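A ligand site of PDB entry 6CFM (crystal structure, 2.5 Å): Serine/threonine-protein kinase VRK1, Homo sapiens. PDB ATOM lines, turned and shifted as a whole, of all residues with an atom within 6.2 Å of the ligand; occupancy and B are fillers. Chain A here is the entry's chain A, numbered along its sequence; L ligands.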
ATOM      1  N   ILE A  43      36.542  28.988  26.173  1.00  0.00           N
ATOM      2  CA  ILE A  43      36.177  29.859  25.043  1.00  0.00           C
ATOM      3  C   ILE A  43      36.349  31.359  25.367  1.00  0.00           C
ATOM      4  O   ILE A  43      36.111  31.776  26.501  1.00  0.00           O
ATOM      5  CB  ILE A  43      34.738  29.598  24.541  1.00  0.00           C
ATOM      6  CG1 ILE A  43      33.674  29.910  25.607  1.00  0.00           C
ATOM      7  CG2 ILE A  43      34.612  28.162  24.042  1.00  0.00           C
ATOM      8  CD1 ILE A  43      32.403  30.499  25.023  1.00  0.00           C
ATOM      9  N   GLY A  44      36.755  32.140  24.348  1.00  0.00           N
ATOM     10  CA  GLY A  44      36.942  33.610  24.424  1.00  0.00           C
ATOM     11  C   GLY A  44      37.033  34.280  25.798  1.00  0.00           C
ATOM     12  O   GLY A  44      38.061  34.205  26.473  1.00  0.00           O
ATOM     13  N   ILE A  51      33.257  27.998  30.739  1.00  0.00           N
ATOM     14  CA  ILE A  51      32.728  27.278  29.595  1.00  0.00           C
ATOM     15  C   ILE A  51      33.919  26.820  28.770  1.00  0.00           C
ATOM     16  O   ILE A  51      34.702  27.650  28.305  1.00  0.00           O
ATOM     17  CB  ILE A  51      31.784  28.169  28.766  1.00  0.00           C
ATOM     18  CG1 ILE A  51      30.699  28.764  29.678  1.00  0.00           C
ATOM     19  CG2 ILE A  51      31.183  27.371  27.615  1.00  0.00           C
ATOM     20  CD1 ILE A  51      29.549  29.449  28.986  1.00  0.00           C
ATOM     21  N   LEU A  53      35.609  24.132  25.670  1.00  0.00           N
ATOM     22  CA  LEU A  53      35.373  23.319  24.499  1.00  0.00           C
ATOM     23  C   LEU A  53      35.309  21.846  24.918  1.00  0.00           C
ATOM     24  O   LEU A  53      35.932  21.440  25.901  1.00  0.00           O
ATOM     25  CB  LEU A  53      36.469  23.544  23.445  1.00  0.00           C
ATOM     26  CG  LEU A  53      36.526  24.971  22.857  1.00  0.00           C
ATOM     27  CD1 LEU A  53      37.875  25.239  22.214  1.00  0.00           C
ATOM     28  CD2 LEU A  53      35.388  25.226  21.870  1.00  0.00           C
ATOM     29  N   SER A  64      40.205  23.599  18.272  1.00  0.00           N
ATOM     30  CA  SER A  64      39.526  24.889  18.071  1.00  0.00           C
ATOM     31  C   SER A  64      38.136  24.728  17.450  1.00  0.00           C
ATOM     32  O   SER A  64      37.242  25.493  17.772  1.00  0.00           O
ATOM     33  CB  SER A  64      40.385  25.807  17.205  1.00  0.00           C
ATOM     34  N   VAL A  69      30.333  22.451  23.959  1.00  0.00           N
ATOM     35  CA  VAL A  69      30.940  23.122  25.092  1.00  0.00           C
ATOM     36  C   VAL A  69      30.507  22.391  26.354  1.00  0.00           C
ATOM     37  O   VAL A  69      29.516  21.697  26.342  1.00  0.00           O
ATOM     38  CB  VAL A  69      30.566  24.627  25.175  1.00  0.00           C
ATOM     39  CG1 VAL A  69      30.979  25.336  23.894  1.00  0.00           C
ATOM     40  CG2 VAL A  69      29.071  24.830  25.457  1.00  0.00           C
ATOM     41  N   LYS A  71      29.696  23.475  30.285  1.00  0.00           N
ATOM     42  CA  LYS A  71      29.522  24.531  31.271  1.00  0.00           C
ATOM     43  C   LYS A  71      29.683  23.893  32.630  1.00  0.00           C
ATOM     44  O   LYS A  71      29.111  22.840  32.875  1.00  0.00           O
ATOM     45  CB  LYS A  71      28.131  25.137  31.152  1.00  0.00           C
ATOM     46  CG  LYS A  71      27.979  25.901  29.851  1.00  0.00           C
ATOM     47  CD  LYS A  71      26.539  26.283  29.548  1.00  0.00           C
ATOM     48  CE  LYS A  71      26.071  27.484  30.350  1.00  0.00           C
ATOM     49  NZ  LYS A  71      25.036  28.243  29.573  1.00  0.00           N
ATOM     50  N   GLU A  83      18.769  26.235  34.318  1.00  0.00           N
ATOM     51  CA  GLU A  83      19.101  26.064  32.909  1.00  0.00           C
ATOM     52  C   GLU A  83      19.183  24.581  32.531  1.00  0.00           C
ATOM     53  O   GLU A  83      18.643  24.173  31.502  1.00  0.00           O
ATOM     54  CB  GLU A  83      20.421  26.747  32.582  1.00  0.00           C
ATOM     55  CG  GLU A  83      20.828  26.642  31.129  1.00  0.00           C
ATOM     56  CD  GLU A  83      21.988  27.538  30.787  1.00  0.00           C
ATOM     57  OE1 GLU A  83      23.076  27.298  31.336  1.00  0.00           O
ATOM     58  OE2 GLU A  83      21.834  28.473  29.980  1.00  0.00           O
ATOM     59  N   TYR A  87      16.892  22.468  29.704  1.00  0.00           N
ATOM     60  CA  TYR A  87      17.515  21.680  28.631  1.00  0.00           C
ATOM     61  C   TYR A  87      17.129  20.191  28.711  1.00  0.00           C
ATOM     62  O   TYR A  87      16.775  19.588  27.705  1.00  0.00           O
ATOM     63  CB  TYR A  87      19.050  21.867  28.617  1.00  0.00           C
ATOM     64  CG  TYR A  87      19.532  23.187  28.007  1.00  0.00           C
ATOM     65  CD1 TYR A  87      19.208  23.548  26.716  1.00  0.00           C
ATOM     66  CD2 TYR A  87      20.351  24.044  28.721  1.00  0.00           C
ATOM     67  CE1 TYR A  87      19.657  24.735  26.153  1.00  0.00           C
ATOM     68  CE2 TYR A  87      20.797  25.227  28.167  1.00  0.00           C
ATOM     69  CZ  TYR A  87      20.449  25.563  26.890  1.00  0.00           C
ATOM     70  OH  TYR A  87      20.904  26.748  26.364  1.00  0.00           O
ATOM     71  N   PRO A 111      19.366  25.361  21.557  1.00  0.00           N
ATOM     72  CA  PRO A 111      20.561  24.523  21.578  1.00  0.00           C
ATOM     73  C   PRO A 111      20.259  23.114  22.087  1.00  0.00           C
ATOM     74  O   PRO A 111      19.369  22.940  22.909  1.00  0.00           O
ATOM     75  CB  PRO A 111      21.494  25.244  22.557  1.00  0.00           C
ATOM     76  CG  PRO A 111      20.936  26.602  22.733  1.00  0.00           C
ATOM     77  CD  PRO A 111      19.461  26.473  22.515  1.00  0.00           C
ATOM     78  N   LYS A 112      21.008  22.131  21.596  1.00  0.00           N
ATOM     79  CA  LYS A 112      20.824  20.746  22.006  1.00  0.00           C
ATOM     80  C   LYS A 112      21.582  20.374  23.294  1.00  0.00           C
ATOM     81  O   LYS A 112      22.762  20.681  23.442  1.00  0.00           O
ATOM     82  CB  LYS A 112      21.230  19.791  20.884  1.00  0.00           C
ATOM     83  CG  LYS A 112      20.305  19.881  19.673  1.00  0.00           C
ATOM     84  CD  LYS A 112      20.526  18.730  18.713  1.00  0.00           C
ATOM     85  CE  LYS A 112      19.444  18.681  17.656  1.00  0.00           C
ATOM     86  NZ  LYS A 112      19.607  19.755  16.634  1.00  0.00           N
ATOM     87  N   MET A 129      27.406  20.498  32.395  1.00  0.00           N
ATOM     88  CA  MET A 129      26.405  20.299  31.358  1.00  0.00           C
ATOM     89  C   MET A 129      27.051  20.438  29.978  1.00  0.00           C
ATOM     90  O   MET A 129      27.771  21.407  29.729  1.00  0.00           O
ATOM     91  CB  MET A 129      25.346  21.382  31.541  1.00  0.00           C
ATOM     92  CG  MET A 129      24.176  21.317  30.563  1.00  0.00           C
ATOM     93  SD  MET A 129      22.976  22.588  30.972  1.00  0.00           S
ATOM     94  CE  MET A 129      23.856  24.063  30.480  1.00  0.00           C
ATOM     95  N   MET A 131      26.578  20.903  25.872  1.00  0.00           N
ATOM     96  CA  MET A 131      25.679  21.661  24.989  1.00  0.00           C
ATOM     97  C   MET A 131      26.343  21.885  23.636  1.00  0.00           C
ATOM     98  O   MET A 131      27.558  21.734  23.518  1.00  0.00           O
ATOM     99  CB  MET A 131      25.428  23.056  25.580  1.00  0.00           C
ATOM    100  CG  MET A 131      24.674  23.102  26.889  1.00  0.00           C
ATOM    101  SD  MET A 131      23.089  22.237  26.858  1.00  0.00           S
ATOM    102  CE  MET A 131      22.283  22.984  25.443  1.00  0.00           C
ATOM    103  N   ASP A 132      25.552  22.313  22.652  1.00  0.00           N
ATOM    104  CA  ASP A 132      26.108  22.716  21.355  1.00  0.00           C
ATOM    105  C   ASP A 132      27.057  23.889  21.488  1.00  0.00           C
ATOM    106  O   ASP A 132      26.893  24.763  22.345  1.00  0.00           O
ATOM    107  CB  ASP A 132      25.003  23.148  20.378  1.00  0.00           C
ATOM    108  CG  ASP A 132      24.139  22.013  19.916  1.00  0.00           C
ATOM    109  OD1 ASP A 132      24.607  20.869  19.916  1.00  0.00           O
ATOM    110  OD2 ASP A 132      22.976  22.275  19.554  1.00  0.00           O
ATOM    111  N   ARG A 133      28.077  23.894  20.634  1.00  0.00           N
ATOM    112  CA  ARG A 133      28.960  25.024  20.459  1.00  0.00           C
ATOM    113  C   ARG A 133      28.435  25.849  19.282  1.00  0.00           C
ATOM    114  O   ARG A 133      27.870  25.297  18.334  1.00  0.00           O
ATOM    115  CB  ARG A 133      30.382  24.541  20.191  1.00  0.00           C
ATOM    116  CG  ARG A 133      31.422  25.641  19.998  1.00  0.00           C
ATOM    117  CD  ARG A 133      31.625  25.973  18.524  1.00  0.00           C
ATOM    118  NE  ARG A 133      32.662  26.974  18.324  1.00  0.00           N
ATOM    119  CZ  ARG A 133      33.973  26.721  18.174  1.00  0.00           C
ATOM    120  NH1 ARG A 133      34.447  25.480  18.197  1.00  0.00           N
ATOM    121  NH2 ARG A 133      34.810  27.736  17.993  1.00  0.00           N
ATOM    122  N   PHE A 134      28.609  27.164  19.366  1.00  0.00           N
ATOM    123  CA  PHE A 134      28.157  28.129  18.349  1.00  0.00           C
ATOM    124  C   PHE A 134      29.266  29.101  17.946  1.00  0.00           C
ATOM    125  O   PHE A 134      30.351  29.089  18.544  1.00  0.00           O
ATOM    126  CB  PHE A 134      26.961  28.903  18.925  1.00  0.00           C
ATOM    127  CG  PHE A 134      25.789  28.028  19.261  1.00  0.00           C
ATOM    128  CD1 PHE A 134      25.053  27.436  18.242  1.00  0.00           C
ATOM    129  CD2 PHE A 134      25.456  27.747  20.585  1.00  0.00           C
ATOM    130  CE1 PHE A 134      23.980  26.612  18.535  1.00  0.00           C
ATOM    131  CE2 PHE A 134      24.375  26.922  20.874  1.00  0.00           C
ATOM    132  CZ  PHE A 134      23.647  26.345  19.854  1.00  0.00           C
ATOM    133  N   GLY A 135      29.006  29.933  16.940  1.00  0.00           N
ATOM    134  CA  GLY A 135      29.940  30.969  16.484  1.00  0.00           C
ATOM    135  C   GLY A 135      29.782  32.256  17.278  1.00  0.00           C
ATOM    136  O   GLY A 135      29.757  32.242  18.509  1.00  0.00           O
ATOM    137  N   SER A 136      29.664  33.377  16.571  1.00  0.00           N
ATOM    138  CA  SER A 136      29.591  34.685  17.216  1.00  0.00           C
ATOM    139  C   SER A 136      28.178  35.005  17.697  1.00  0.00           C
ATOM    140  O   SER A 136      27.203  34.601  17.072  1.00  0.00           O
ATOM    141  CB  SER A 136      30.050  35.770  16.246  1.00  0.00           C
ATOM    142  OG  SER A 136      30.046  37.043  16.897  1.00  0.00           O
ATOM    143  N   ASP A 137      28.088  35.744  18.806  1.00  0.00           N
ATOM    144  CA  ASP A 137      26.823  36.383  19.213  1.00  0.00           C
ATOM    145  C   ASP A 137      26.467  37.550  18.279  1.00  0.00           C
ATOM    146  O   ASP A 137      27.355  38.151  17.658  1.00  0.00           O
ATOM    147  CB  ASP A 137      26.829  36.851  20.676  1.00  0.00           C
ATOM    148  CG  ASP A 137      27.959  37.801  20.981  1.00  0.00           C
ATOM    149  OD1 ASP A 137      29.076  37.296  21.233  1.00  0.00           O
ATOM    150  OD2 ASP A 137      27.744  39.032  20.976  1.00  0.00           O
ATOM    151  N   SER A 181      22.890  39.686  22.463  1.00  0.00           N
ATOM    152  CA  SER A 181      23.980  38.940  23.088  1.00  0.00           C
ATOM    153  C   SER A 181      23.573  37.518  23.541  1.00  0.00           C
ATOM    154  O   SER A 181      24.439  36.671  23.783  1.00  0.00           O
ATOM    155  CB  SER A 181      24.632  39.739  24.223  1.00  0.00           C
ATOM    156  OG  SER A 181      23.887  39.686  25.424  1.00  0.00           O
ATOM    157  N   LEU A 184      23.159  33.502  19.227  1.00  0.00           N
ATOM    158  CA  LEU A 184      24.416  32.991  18.695  1.00  0.00           C
ATOM    159  C   LEU A 184      24.168  32.365  17.334  1.00  0.00           C
ATOM    160  O   LEU A 184      23.175  31.671  17.155  1.00  0.00           O
ATOM    161  CB  LEU A 184      25.007  31.937  19.631  1.00  0.00           C
ATOM    162  CG  LEU A 184      25.155  32.312  21.107  1.00  0.00           C
ATOM    163  CD1 LEU A 184      25.990  31.281  21.858  1.00  0.00           C
ATOM    164  CD2 LEU A 184      25.755  33.691  21.307  1.00  0.00           C
ATOM    165  N   VAL A 196      20.074  31.373  23.449  1.00  0.00           N
ATOM    166  CA  VAL A 196      20.808  30.680  24.533  1.00  0.00           C
ATOM    167  C   VAL A 196      20.549  31.373  25.866  1.00  0.00           C
ATOM    168  O   VAL A 196      19.861  32.390  25.909  1.00  0.00           O
ATOM    169  CB  VAL A 196      22.345  30.614  24.256  1.00  0.00           C
ATOM    170  CG1 VAL A 196      22.617  30.114  22.852  1.00  0.00           C
ATOM    171  CG2 VAL A 196      23.036  31.965  24.461  1.00  0.00           C
ATOM    172  N   ASP A 197      21.102  30.804  26.939  1.00  0.00           N
ATOM    173  CA  ASP A 197      21.015  31.359  28.307  1.00  0.00           C
ATOM    174  C   ASP A 197      19.627  31.202  28.924  1.00  0.00           C
ATOM    175  O   ASP A 197      18.788  32.099  28.802  1.00  0.00           O
ATOM    176  CB  ASP A 197      21.455  32.821  28.339  1.00  0.00           C
ATOM    177  CG  ASP A 197      21.778  33.314  29.727  1.00  0.00           C
ATOM    178  OD1 ASP A 197      21.183  32.831  30.718  1.00  0.00           O
ATOM    179  OD2 ASP A 197      22.642  34.212  29.827  1.00  0.00           O
ATOM    180  N   TYR A 198      19.398  30.068  29.594  1.00  0.00           N
ATOM    181  CA  TYR A 198      18.122  29.797  30.250  1.00  0.00           C
ATOM    182  C   TYR A 198      18.272  29.759  31.769  1.00  0.00           C
ATOM    183  O   TYR A 198      17.414  29.224  32.448  1.00  0.00           O
ATOM    184  CB  TYR A 198      17.504  28.491  29.691  1.00  0.00           C
ATOM    185  CG  TYR A 198      17.144  28.608  28.221  1.00  0.00           C
ATOM    186  CD1 TYR A 198      18.109  28.435  27.229  1.00  0.00           C
ATOM    187  CD2 TYR A 198      15.854  28.933  27.822  1.00  0.00           C
ATOM    188  CE1 TYR A 198      17.802  28.579  25.876  1.00  0.00           C
ATOM    189  CE2 TYR A 198      15.524  29.078  26.473  1.00  0.00           C
ATOM    190  CZ  TYR A 198      16.504  28.904  25.498  1.00  0.00           C
ATOM    191  OH  TYR A 198      16.203  29.044  24.157  1.00  0.00           O
HETATM  192  C1  LIG L   1      30.323  33.027  22.931  1.00  0.00           C
HETATM  193  C2  LIG L   1      32.202  30.863  20.367  1.00  0.00           C
HETATM  194  C3  LIG L   1      28.589  28.567  23.146  1.00  0.00           C
HETATM  195  C4  LIG L   1      30.228  28.973  21.576  1.00  0.00           C
HETATM  196  C5  LIG L   1      24.529  26.985  25.360  1.00  0.00           C
HETATM  197  C6  LIG L   1      26.594  27.869  24.553  1.00  0.00           C
HETATM  198  C7  LIG L   1      26.460  28.955  25.414  1.00  0.00           C
HETATM  199  C8  LIG L   1      25.338  29.038  26.218  1.00  0.00           C
HETATM  200  C9  LIG L   1      24.353  28.070  26.217  1.00  0.00           C
HETATM  201  C10 LIG L   1      25.621  26.879  24.532  1.00  0.00           C
HETATM  202  C11 LIG L   1      29.301  33.992  22.352  1.00  0.00           C
HETATM  203  N1  LIG L   1      29.612  31.950  23.672  1.00  0.00           N
HETATM  204  N2  LIG L   1      31.306  31.250  21.474  1.00  0.00           N
HETATM  205  C12 LIG L   1      31.303  32.563  21.861  1.00  0.00           C
HETATM  206  N3  LIG L   1      28.667  29.804  23.677  1.00  0.00           N
HETATM  207  C13 LIG L   1      29.549  30.671  23.148  1.00  0.00           C
HETATM  208  C14 LIG L   1      30.393  30.296  22.052  1.00  0.00           C
HETATM  209  N4  LIG L   1      29.349  28.139  22.111  1.00  0.00           N
HETATM  210  N5  LIG L   1      27.703  27.682  23.688  1.00  0.00           N
HETATM  211  O1  LIG L   1      32.062  33.378  21.356  1.00  0.00           O
HETATM  212  C15 LIG L   1      33.491  30.280  20.759  1.00  0.00           C
HETATM  213  C16 LIG L   1      34.502  29.710  20.998  1.00  0.00           C
HETATM  214  C17 LIG L   1      28.934  32.293  24.929  1.00  0.00           C
HETATM  215  F1  LIG L   1      23.595  26.004  25.322  1.00  0.00           F
HETATM  216  O2  LIG L   1      23.276  28.214  27.047  1.00  0.00           O
HETATM  217  F2  LIG L   1      25.198  30.099  27.052  1.00  0.00           F
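O of Gly 135 lies close to N2 of the ligand, at 3.5 Å. Residues that only touch the ligand: Met 131, Ile 43, Asp 137, Arg 133, Pro 111, Leu 184, Val 69 and Val 196. Of the 24 residues printed, 15 come within 4 Å of the ligand. The nearest printed residue that does not touch the ligand is Leu 53 (4.7 Å).
NZ of Lys 71 is in salt-bridge range of OE1 of Glu 83 (2.8 Å). The backbone NH (N) of Lys 71 is in hydrogen-bond range of the backbone carbonyl oxygen (O) of Met 129 (2.9 Å). The backbone NH of Tyr 198 lies within hydrogen-bond range of the side-chain carboxylate of Glu 83, at 2.9 Å. O of Met 131 is in hydrogen-bond range of N of Val 69. The side-chain carboxylate (OD2) of Asp 132 sits at hydrogen-bond distance from the backbone NH (N) of Lys 112, at 2.8 Å. The backbone NH of Ile 43 lies within hydrogen-bond range of the backbone carbonyl oxygen of Ile 51. O of Ser 64 lies within hydrogen-bond range of NH1 of Arg 133 (2.8 Å).
The side-chain hydroxyl (OH) of Tyr 87 lies within hydrogen-bond range of an oxygen (O2) of the ligand, at 2.9 Å. The backbone NH of Phe 134 sits at hydrogen-bond distance from a nitrogen (N4) of the ligand, 3.0 Å away. The side-chain amino group of Lys 71 sits at hydrogen-bond distance from an oxygen (O2) of the ligand, at 3.1 Å. OE2 of Glu 83 is in hydrogen-bond range of O2 of the ligand, at 3.3 Å. The backbone carbonyl oxygen of Asp 132 lies close to a nitrogen (N5) of the ligand (3.3 Å). N of Asp 197 sits at hydrogen-bond distance from O2 of the ligand, at 3.4 Å.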
